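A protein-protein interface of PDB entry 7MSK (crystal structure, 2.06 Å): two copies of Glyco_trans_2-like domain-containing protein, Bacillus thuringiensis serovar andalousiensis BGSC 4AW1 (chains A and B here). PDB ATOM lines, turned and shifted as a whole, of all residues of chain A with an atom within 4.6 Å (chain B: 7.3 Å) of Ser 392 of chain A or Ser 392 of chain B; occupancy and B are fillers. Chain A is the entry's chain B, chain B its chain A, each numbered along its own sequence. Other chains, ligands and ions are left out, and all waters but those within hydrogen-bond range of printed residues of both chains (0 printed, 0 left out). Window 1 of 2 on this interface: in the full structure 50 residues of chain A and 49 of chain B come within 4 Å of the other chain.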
ATOM      1  N   PHE A 348      11.645   8.262  38.096  1.00  0.00           N
ATOM      2  CA  PHE A 348      11.745   7.800  36.716  1.00  0.00           C
ATOM      3  C   PHE A 348      10.639   8.410  35.863  1.00  0.00           C
ATOM      4  O   PHE A 348      10.866   8.777  34.707  1.00  0.00           O
ATOM      5  CB  PHE A 348      11.739   6.272  36.653  1.00  0.00           C
ATOM      6  CG  PHE A 348      11.892   5.673  35.276  1.00  0.00           C
ATOM      7  CD1 PHE A 348      12.740   6.234  34.331  1.00  0.00           C
ATOM      8  CD2 PHE A 348      11.221   4.505  34.939  1.00  0.00           C
ATOM      9  CE1 PHE A 348      12.896   5.660  33.079  1.00  0.00           C
ATOM     10  CE2 PHE A 348      11.359   3.940  33.678  1.00  0.00           C
ATOM     11  CZ  PHE A 348      12.212   4.509  32.758  1.00  0.00           C
ATOM     12  N   THR A 355      12.162  14.001  29.228  1.00  0.00           N
ATOM     13  CA  THR A 355      12.635  13.524  27.940  1.00  0.00           C
ATOM     14  C   THR A 355      11.571  13.780  26.876  1.00  0.00           C
ATOM     15  O   THR A 355      11.886  14.240  25.785  1.00  0.00           O
ATOM     16  CB  THR A 355      13.087  12.063  28.030  1.00  0.00           C
ATOM     17  OG1 THR A 355      13.958  11.930  29.152  1.00  0.00           O
ATOM     18  CG2 THR A 355      13.812  11.593  26.789  1.00  0.00           C
ATOM     19  N   GLU A 388      16.849   8.368  19.354  1.00  0.00           N
ATOM     20  CA  GLU A 388      17.384   8.005  20.658  1.00  0.00           C
ATOM     21  C   GLU A 388      16.413   8.430  21.759  1.00  0.00           C
ATOM     22  O   GLU A 388      16.218   7.698  22.719  1.00  0.00           O
ATOM     23  CB  GLU A 388      18.760   8.640  20.894  1.00  0.00           C
ATOM     24  CG  GLU A 388      19.842   8.134  19.951  1.00  0.00           C
ATOM     25  CD  GLU A 388      19.945   6.623  19.924  1.00  0.00           C
ATOM     26  OE1 GLU A 388      20.190   6.035  21.001  1.00  0.00           O
ATOM     27  OE2 GLU A 388      19.723   6.027  18.836  1.00  0.00           O
ATOM     28  N   LEU A 389      15.802   9.610  21.640  1.00  0.00           N
ATOM     29  CA  LEU A 389      14.855  10.046  22.661  1.00  0.00           C
ATOM     30  C   LEU A 389      13.641   9.104  22.703  1.00  0.00           C
ATOM     31  O   LEU A 389      13.230   8.670  23.778  1.00  0.00           O
ATOM     32  CB  LEU A 389      14.466  11.505  22.407  1.00  0.00           C
ATOM     33  CG  LEU A 389      15.581  12.541  22.594  1.00  0.00           C
ATOM     34  CD1 LEU A 389      15.121  13.908  22.124  1.00  0.00           C
ATOM     35  CD2 LEU A 389      16.052  12.616  24.043  1.00  0.00           C
ATOM     36  N   TYR A 390      13.120   8.717  21.529  1.00  0.00           N
ATOM     37  CA  TYR A 390      12.012   7.771  21.439  1.00  0.00           C
ATOM     38  C   TYR A 390      12.314   6.453  22.148  1.00  0.00           C
ATOM     39  O   TYR A 390      11.470   5.952  22.895  1.00  0.00           O
ATOM     40  CB  TYR A 390      11.655   7.500  19.977  1.00  0.00           C
ATOM     41  CG  TYR A 390      10.766   8.541  19.347  1.00  0.00           C
ATOM     42  CD1 TYR A 390       9.614   8.984  19.986  1.00  0.00           C
ATOM     43  CD2 TYR A 390      11.052   9.063  18.101  1.00  0.00           C
ATOM     44  CE1 TYR A 390       8.787   9.937  19.414  1.00  0.00           C
ATOM     45  CE2 TYR A 390      10.229  10.006  17.511  1.00  0.00           C
ATOM     46  CZ  TYR A 390       9.095  10.446  18.169  1.00  0.00           C
ATOM     47  OH  TYR A 390       8.294  11.383  17.594  1.00  0.00           O
ATOM     48  N   CYS A 391      13.497   5.872  21.907  1.00  0.00           N
ATOM     49  CA  CYS A 391      13.858   4.614  22.548  1.00  0.00           C
ATOM     50  C   CYS A 391      14.000   4.801  24.052  1.00  0.00           C
ATOM     51  O   CYS A 391      13.662   3.905  24.834  1.00  0.00           O
ATOM     52  CB  CYS A 391      15.156   4.043  21.993  1.00  0.00           C
ATOM     53  SG  CYS A 391      14.999   3.510  20.269  1.00  0.00           S
ATOM     54  N   SER A 392      14.496   5.976  24.446  1.00  0.00           N
ATOM     55  CA  SER A 392      14.701   6.285  25.852  1.00  0.00           C
ATOM     56  C   SER A 392      13.383   6.229  26.626  1.00  0.00           C
ATOM     57  O   SER A 392      13.364   5.780  27.769  1.00  0.00           O
ATOM     58  CB  SER A 392      15.357   7.626  26.010  1.00  0.00           C
ATOM     59  OG  SER A 392      15.835   7.772  27.329  1.00  0.00           O
ATOM     60  N   ILE A 393      12.291   6.706  26.015  1.00  0.00           N
ATOM     61  CA  ILE A 393      11.007   6.703  26.707  1.00  0.00           C
ATOM     62  C   ILE A 393      10.169   5.483  26.330  1.00  0.00           C
ATOM     63  O   ILE A 393       8.984   5.472  26.646  1.00  0.00           O
ATOM     64  CB  ILE A 393      10.218   8.010  26.484  1.00  0.00           C
ATOM     65  CG1 ILE A 393       9.905   8.268  25.007  1.00  0.00           C
ATOM     66  CG2 ILE A 393      10.952   9.186  27.130  1.00  0.00           C
ATOM     67  CD1 ILE A 393       8.900   9.384  24.784  1.00  0.00           C
ATOM     68  N   ASP A 394      10.775   4.476  25.677  1.00  0.00           N
ATOM     69  CA  ASP A 394      10.114   3.218  25.343  1.00  0.00           C
ATOM     70  C   ASP A 394       8.966   3.449  24.354  1.00  0.00           C
ATOM     71  O   ASP A 394       7.961   2.745  24.413  1.00  0.00           O
ATOM     72  CB  ASP A 394       9.602   2.495  26.597  1.00  0.00           C
ATOM     73  CG  ASP A 394       8.983   1.131  26.314  1.00  0.00           C
ATOM     74  OD1 ASP A 394       9.419   0.487  25.345  1.00  0.00           O
ATOM     75  OD2 ASP A 394       8.081   0.709  27.083  1.00  0.00           O
ATOM     76  N   PHE B 348      19.949  15.887  26.870  1.00  0.00           N
ATOM     77  CA  PHE B 348      19.803  14.441  26.796  1.00  0.00           C
ATOM     78  C   PHE B 348      20.910  13.734  27.576  1.00  0.00           C
ATOM     79  O   PHE B 348      20.643  12.772  28.295  1.00  0.00           O
ATOM     80  CB  PHE B 348      19.770  13.952  25.345  1.00  0.00           C
ATOM     81  CG  PHE B 348      19.528  12.473  25.182  1.00  0.00           C
ATOM     82  CD1 PHE B 348      18.651  11.793  26.017  1.00  0.00           C
ATOM     83  CD2 PHE B 348      20.184  11.755  24.196  1.00  0.00           C
ATOM     84  CE1 PHE B 348      18.420  10.435  25.854  1.00  0.00           C
ATOM     85  CE2 PHE B 348      19.965  10.395  24.046  1.00  0.00           C
ATOM     86  CZ  PHE B 348      19.071   9.740  24.866  1.00  0.00           C
ATOM     87  N   ILE B 351      20.209  13.973  31.248  1.00  0.00           N
ATOM     88  CA  ILE B 351      19.104  13.101  31.611  1.00  0.00           C
ATOM     89  C   ILE B 351      19.607  11.670  31.785  1.00  0.00           C
ATOM     90  O   ILE B 351      19.211  10.995  32.731  1.00  0.00           O
ATOM     91  CB  ILE B 351      17.954  13.176  30.583  1.00  0.00           C
ATOM     92  CG1 ILE B 351      17.130  14.450  30.773  1.00  0.00           C
ATOM     93  CG2 ILE B 351      17.072  11.931  30.644  1.00  0.00           C
ATOM     94  CD1 ILE B 351      16.299  14.814  29.574  1.00  0.00           C
ATOM     95  N   ARG B 352      20.455  11.198  30.868  1.00  0.00           N
ATOM     96  CA  ARG B 352      20.952   9.837  30.935  1.00  0.00           C
ATOM     97  C   ARG B 352      21.817   9.638  32.174  1.00  0.00           C
ATOM     98  O   ARG B 352      21.804   8.552  32.747  1.00  0.00           O
ATOM     99  CB  ARG B 352      21.752   9.493  29.681  1.00  0.00           C
ATOM    100  CG  ARG B 352      20.902   9.396  28.426  1.00  0.00           C
ATOM    101  CD  ARG B 352      21.761   9.154  27.206  1.00  0.00           C
ATOM    102  NE  ARG B 352      22.386   7.847  27.278  1.00  0.00           N
ATOM    103  CZ  ARG B 352      22.241   6.874  26.387  1.00  0.00           C
ATOM    104  NH1 ARG B 352      21.489   7.034  25.308  1.00  0.00           N
ATOM    105  NH2 ARG B 352      22.870   5.730  26.577  1.00  0.00           N
ATOM    106  N   THR B 355      19.492   9.182  35.014  1.00  0.00           N
ATOM    107  CA  THR B 355      18.897   7.855  34.973  1.00  0.00           C
ATOM    108  C   THR B 355      19.907   6.826  35.499  1.00  0.00           C
ATOM    109  O   THR B 355      19.551   5.904  36.235  1.00  0.00           O
ATOM    110  CB  THR B 355      18.357   7.524  33.568  1.00  0.00           C
ATOM    111  OG1 THR B 355      17.539   8.573  33.036  1.00  0.00           O
ATOM    112  CG2 THR B 355      17.509   6.273  33.546  1.00  0.00           C
ATOM    113  N   LEU B 386      14.652  -1.788  37.274  1.00  0.00           N
ATOM    114  CA  LEU B 386      16.043  -1.618  36.867  1.00  0.00           C
ATOM    115  C   LEU B 386      16.214  -1.952  35.387  1.00  0.00           C
ATOM    116  O   LEU B 386      16.954  -1.264  34.689  1.00  0.00           O
ATOM    117  CB  LEU B 386      16.956  -2.501  37.730  1.00  0.00           C
ATOM    118  CG  LEU B 386      17.044  -2.112  39.206  1.00  0.00           C
ATOM    119  CD1 LEU B 386      17.761  -3.181  40.026  1.00  0.00           C
ATOM    120  CD2 LEU B 386      17.719  -0.755  39.377  1.00  0.00           C
ATOM    121  N   ILE B 387      15.543  -3.010  34.919  1.00  0.00           N
ATOM    122  CA  ILE B 387      15.585  -3.378  33.512  1.00  0.00           C
ATOM    123  C   ILE B 387      15.059  -2.228  32.658  1.00  0.00           C
ATOM    124  O   ILE B 387      15.619  -1.947  31.598  1.00  0.00           O
ATOM    125  CB  ILE B 387      14.804  -4.681  33.262  1.00  0.00           C
ATOM    126  CG1 ILE B 387      15.500  -5.866  33.938  1.00  0.00           C
ATOM    127  CG2 ILE B 387      14.592  -4.924  31.767  1.00  0.00           C
ATOM    128  CD1 ILE B 387      14.577  -7.014  34.275  1.00  0.00           C
ATOM    129  N   GLU B 388      13.979  -1.570  33.116  1.00  0.00           N
ATOM    130  CA  GLU B 388      13.428  -0.422  32.405  1.00  0.00           C
ATOM    131  C   GLU B 388      14.490   0.674  32.312  1.00  0.00           C
ATOM    132  O   GLU B 388      14.674   1.290  31.262  1.00  0.00           O
ATOM    133  CB  GLU B 388      12.160   0.111  33.098  1.00  0.00           C
ATOM    134  CG  GLU B 388      10.948  -0.792  32.963  1.00  0.00           C
ATOM    135  CD  GLU B 388      10.746  -1.277  31.543  1.00  0.00           C
ATOM    136  OE1 GLU B 388      10.494  -0.436  30.674  1.00  0.00           O
ATOM    137  OE2 GLU B 388      10.915  -2.486  31.300  1.00  0.00           O
ATOM    138  N   LEU B 389      15.175   0.925  33.431  1.00  0.00           N
ATOM    139  CA  LEU B 389      16.185   1.973  33.483  1.00  0.00           C
ATOM    140  C   LEU B 389      17.342   1.635  32.543  1.00  0.00           C
ATOM    141  O   LEU B 389      17.822   2.510  31.828  1.00  0.00           O
ATOM    142  CB  LEU B 389      16.659   2.149  34.932  1.00  0.00           C
ATOM    143  CG  LEU B 389      15.613   2.652  35.927  1.00  0.00           C
ATOM    144  CD1 LEU B 389      16.193   2.670  37.334  1.00  0.00           C
ATOM    145  CD2 LEU B 389      15.082   4.031  35.553  1.00  0.00           C
ATOM    146  N   TYR B 390      17.774   0.366  32.524  1.00  0.00           N
ATOM    147  CA  TYR B 390      18.826  -0.080  31.611  1.00  0.00           C
ATOM    148  C   TYR B 390      18.472   0.252  30.163  1.00  0.00           C
ATOM    149  O   TYR B 390      19.279   0.850  29.467  1.00  0.00           O
ATOM    150  CB  TYR B 390      19.100  -1.584  31.748  1.00  0.00           C
ATOM    151  CG  TYR B 390      20.028  -1.953  32.879  1.00  0.00           C
ATOM    152  CD1 TYR B 390      21.338  -1.501  32.910  1.00  0.00           C
ATOM    153  CD2 TYR B 390      19.596  -2.752  33.922  1.00  0.00           C
ATOM    154  CE1 TYR B 390      22.195  -1.831  33.948  1.00  0.00           C
ATOM    155  CE2 TYR B 390      20.433  -3.079  34.976  1.00  0.00           C
ATOM    156  CZ  TYR B 390      21.740  -2.623  34.987  1.00  0.00           C
ATOM    157  OH  TYR B 390      22.557  -2.963  36.031  1.00  0.00           O
ATOM    158  N   CYS B 391      17.265  -0.135  29.719  1.00  0.00           N
ATOM    159  CA  CYS B 391      16.812   0.115  28.354  1.00  0.00           C
ATOM    160  C   CYS B 391      16.769   1.612  28.046  1.00  0.00           C
ATOM    161  O   CYS B 391      17.158   2.042  26.969  1.00  0.00           O
ATOM    162  CB  CYS B 391      15.423  -0.474  28.112  1.00  0.00           C
ATOM    163  SG  CYS B 391      15.318  -2.261  28.394  1.00  0.00           S
ATOM    164  N   SER B 392      16.283   2.415  28.996  1.00  0.00           N
ATOM    165  CA  SER B 392      16.165   3.850  28.794  1.00  0.00           C
ATOM    166  C   SER B 392      17.516   4.470  28.411  1.00  0.00           C
ATOM    167  O   SER B 392      17.568   5.406  27.607  1.00  0.00           O
ATOM    168  CB  SER B 392      15.603   4.492  30.026  1.00  0.00           C
ATOM    169  OG  SER B 392      15.469   5.885  29.843  1.00  0.00           O
ATOM    170  N   ILE B 393      18.601   3.963  29.017  1.00  0.00           N
ATOM    171  CA  ILE B 393      19.927   4.515  28.795  1.00  0.00           C
ATOM    172  C   ILE B 393      20.696   3.644  27.805  1.00  0.00           C
ATOM    173  O   ILE B 393      21.915   3.725  27.753  1.00  0.00           O
ATOM    174  CB  ILE B 393      20.705   4.664  30.120  1.00  0.00           C
ATOM    175  CG1 ILE B 393      21.132   3.308  30.698  1.00  0.00           C
ATOM    176  CG2 ILE B 393      19.909   5.482  31.125  1.00  0.00           C
ATOM    177  CD1 ILE B 393      22.002   3.410  31.927  1.00  0.00           C
ATOM    178  N   ASP B 394      19.986   2.788  27.063  1.00  0.00           N
ATOM    179  CA  ASP B 394      20.555   2.034  25.956  1.00  0.00           C
ATOM    180  C   ASP B 394      21.657   1.086  26.450  1.00  0.00           C
ATOM    181  O   ASP B 394      22.691   0.967  25.810  1.00  0.00           O
ATOM    182  CB  ASP B 394      21.032   3.002  24.862  1.00  0.00           C
ATOM    183  CG  ASP B 394      21.522   2.328  23.593  1.00  0.00           C
ATOM    184  OD1 ASP B 394      21.046   1.230  23.300  1.00  0.00           O
ATOM    185  OD2 ASP B 394      22.362   2.924  22.891  1.00  0.00           O
ATOM    186  N   ASP B 395      21.438   0.407  27.584  1.00  0.00           N
ATOM    187  CA  ASP B 395      22.355  -0.610  28.085  1.00  0.00           C
ATOM    188  C   ASP B 395      21.627  -1.950  28.136  1.00  0.00           C
ATOM    189  O   ASP B 395      21.278  -2.441  29.207  1.00  0.00           O
ATOM    190  CB  ASP B 395      22.909  -0.220  29.457  1.00  0.00           C
ATOM    191  CG  ASP B 395      23.857  -1.241  30.068  1.00  0.00           C
ATOM    192  OD1 ASP B 395      24.127  -2.257  29.404  1.00  0.00           O
ATOM    193  OD2 ASP B 395      24.307  -1.014  31.209  1.00  0.00           O
ATOM    194  N   TRP B 396      21.418  -2.544  26.961  1.00  0.00           N
ATOM    195  CA  TRP B 396      20.543  -3.698  26.814  1.00  0.00           C
ATOM    196  C   TRP B 396      21.137  -4.960  27.437  1.00  0.00           C
ATOM    197  O   TRP B 396      20.398  -5.830  27.901  1.00  0.00           O
ATOM    198  CB  TRP B 396      20.215  -3.897  25.332  1.00  0.00           C
ATOM    199  CG  TRP B 396      19.096  -3.015  24.877  1.00  0.00           C
ATOM    200  CD1 TRP B 396      19.172  -1.729  24.429  1.00  0.00           C
ATOM    201  CD2 TRP B 396      17.702  -3.361  24.875  1.00  0.00           C
ATOM    202  NE1 TRP B 396      17.923  -1.259  24.128  1.00  0.00           N
ATOM    203  CE2 TRP B 396      17.001  -2.236  24.396  1.00  0.00           C
ATOM    204  CE3 TRP B 396      16.988  -4.514  25.224  1.00  0.00           C
ATOM    205  CZ2 TRP B 396      15.615  -2.237  24.253  1.00  0.00           C
ATOM    206  CZ3 TRP B 396      15.620  -4.515  25.079  1.00  0.00           C
ATOM    207  CH2 TRP B 396      14.948  -3.389  24.601  1.00  0.00           C
ATOM    208  N   ARG B 418       7.960  -5.552  24.675  1.00  0.00           N
ATOM    209  CA  ARG B 418       8.869  -4.641  23.997  1.00  0.00           C
ATOM    210  C   ARG B 418       9.642  -5.404  22.922  1.00  0.00           C
ATOM    211  O   ARG B 418       9.699  -4.972  21.776  1.00  0.00           O
ATOM    212  CB  ARG B 418       9.863  -3.997  24.972  1.00  0.00           C
ATOM    213  CG  ARG B 418      10.176  -2.539  24.658  1.00  0.00           C
ATOM    214  CD  ARG B 418      11.468  -2.019  25.263  1.00  0.00           C
ATOM    215  NE  ARG B 418      11.763  -2.553  26.584  1.00  0.00           N
ATOM    216  CZ  ARG B 418      11.180  -2.180  27.723  1.00  0.00           C
ATOM    217  NH1 ARG B 418      10.233  -1.257  27.737  1.00  0.00           N
ATOM    218  NH2 ARG B 418      11.547  -2.744  28.856  1.00  0.00           N
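Phe 348 of chain A touches Glu 388 of chain B, and with the chains exchanged Glu 388 of chain A touches Phe 348 of chain B. Phe 348 of chain A touches Leu 389 of chain B, and with the chains exchanged Leu 389 of chain A touches Phe 348 of chain B. Ser 392 of chain A touches Phe 348 of chain B, but with the chains exchanged Phe 348 of chain A does not touch Ser 392 of chain B (4.1 Å). Ser 392 of chain A touches its own counterpart, Ser 392 of chain B. Of the 8 pairs that touch across the chains among the printed residues, 5 have their exchanged pair printed and touching as well.
The backbone carbonyl oxygen (O) of Ser 392 of chain B lies within hydrogen-bond range of the side-chain hydroxyl (OG) of Ser 392 of chain A (2.9 Å). The guanidinium group (NH1) of Arg 418 of chain B is in salt-bridge range of the side-chain carboxylate (OD2) of Asp 394 of chain A.
O of Ile 351 of chain B lies within hydrogen-bond range of OG1 of Thr 355 of chain B, at 3.0 Å. OE2 of Glu 388 of chain B is in salt-bridge range of NH2 of Arg 418 of chain B (2.5 Å).
Printed residues of chain A that touch a printed residue of chain B: Phe 348, Thr 355, Glu 388, Leu 389, Ser 392 and Asp 394. Hydrophobic or aromatic side chains of chain A within 4 Å of the printed part of chain B: Phe 348 and Leu 389. Among the printed residues, 8 pairs touch across the chains. Among the printed residues, Asp or Glu carboxylates within 4 Å of a Lys or Arg side-chain nitrogen of the other chain: Asp 394 of chain A with Arg 418 of chain B (3.0 Å).
Among the printed residues, pairs that only touch across the chains: Phe 348 of chain A with Glu 388 of chain B, Phe 348 of chain A with Leu 389 of chain B, Thr 355 of chain A with Ile 351 of chain B, Glu 388 of chain A with Phe 348 of chain B, Leu 389 of chain A with Phe 348 of chain B and Ser 392 of chain A with Phe 348 of chain B.
Of the printed residues of chain B, Ser 392 of chain A touches Phe 348 (3.99 Å) and Ser 392 (2.9 Å). Ser 392 of chain B touches just one residue of chain A: Ser 392. Printed residues of chain B within 4 Å of Phe 348 of chain A: Glu 388 (3.95 Å) and Leu 389 (3.4 Å). Of the printed residues of chain A, Ile 351 of chain B touches Thr 355 (3.5 Å). Tyr 390 of chain A touches none of the printed residues of chain B. The nearest residue of chain A that does not touch Ser 392 of chain B is Phe 348 of chain A (4.1 Å). The nearest printed residue of chain B that does not touch Asp 394 of chain A is Glu 388 of chain B (4.5 Å).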
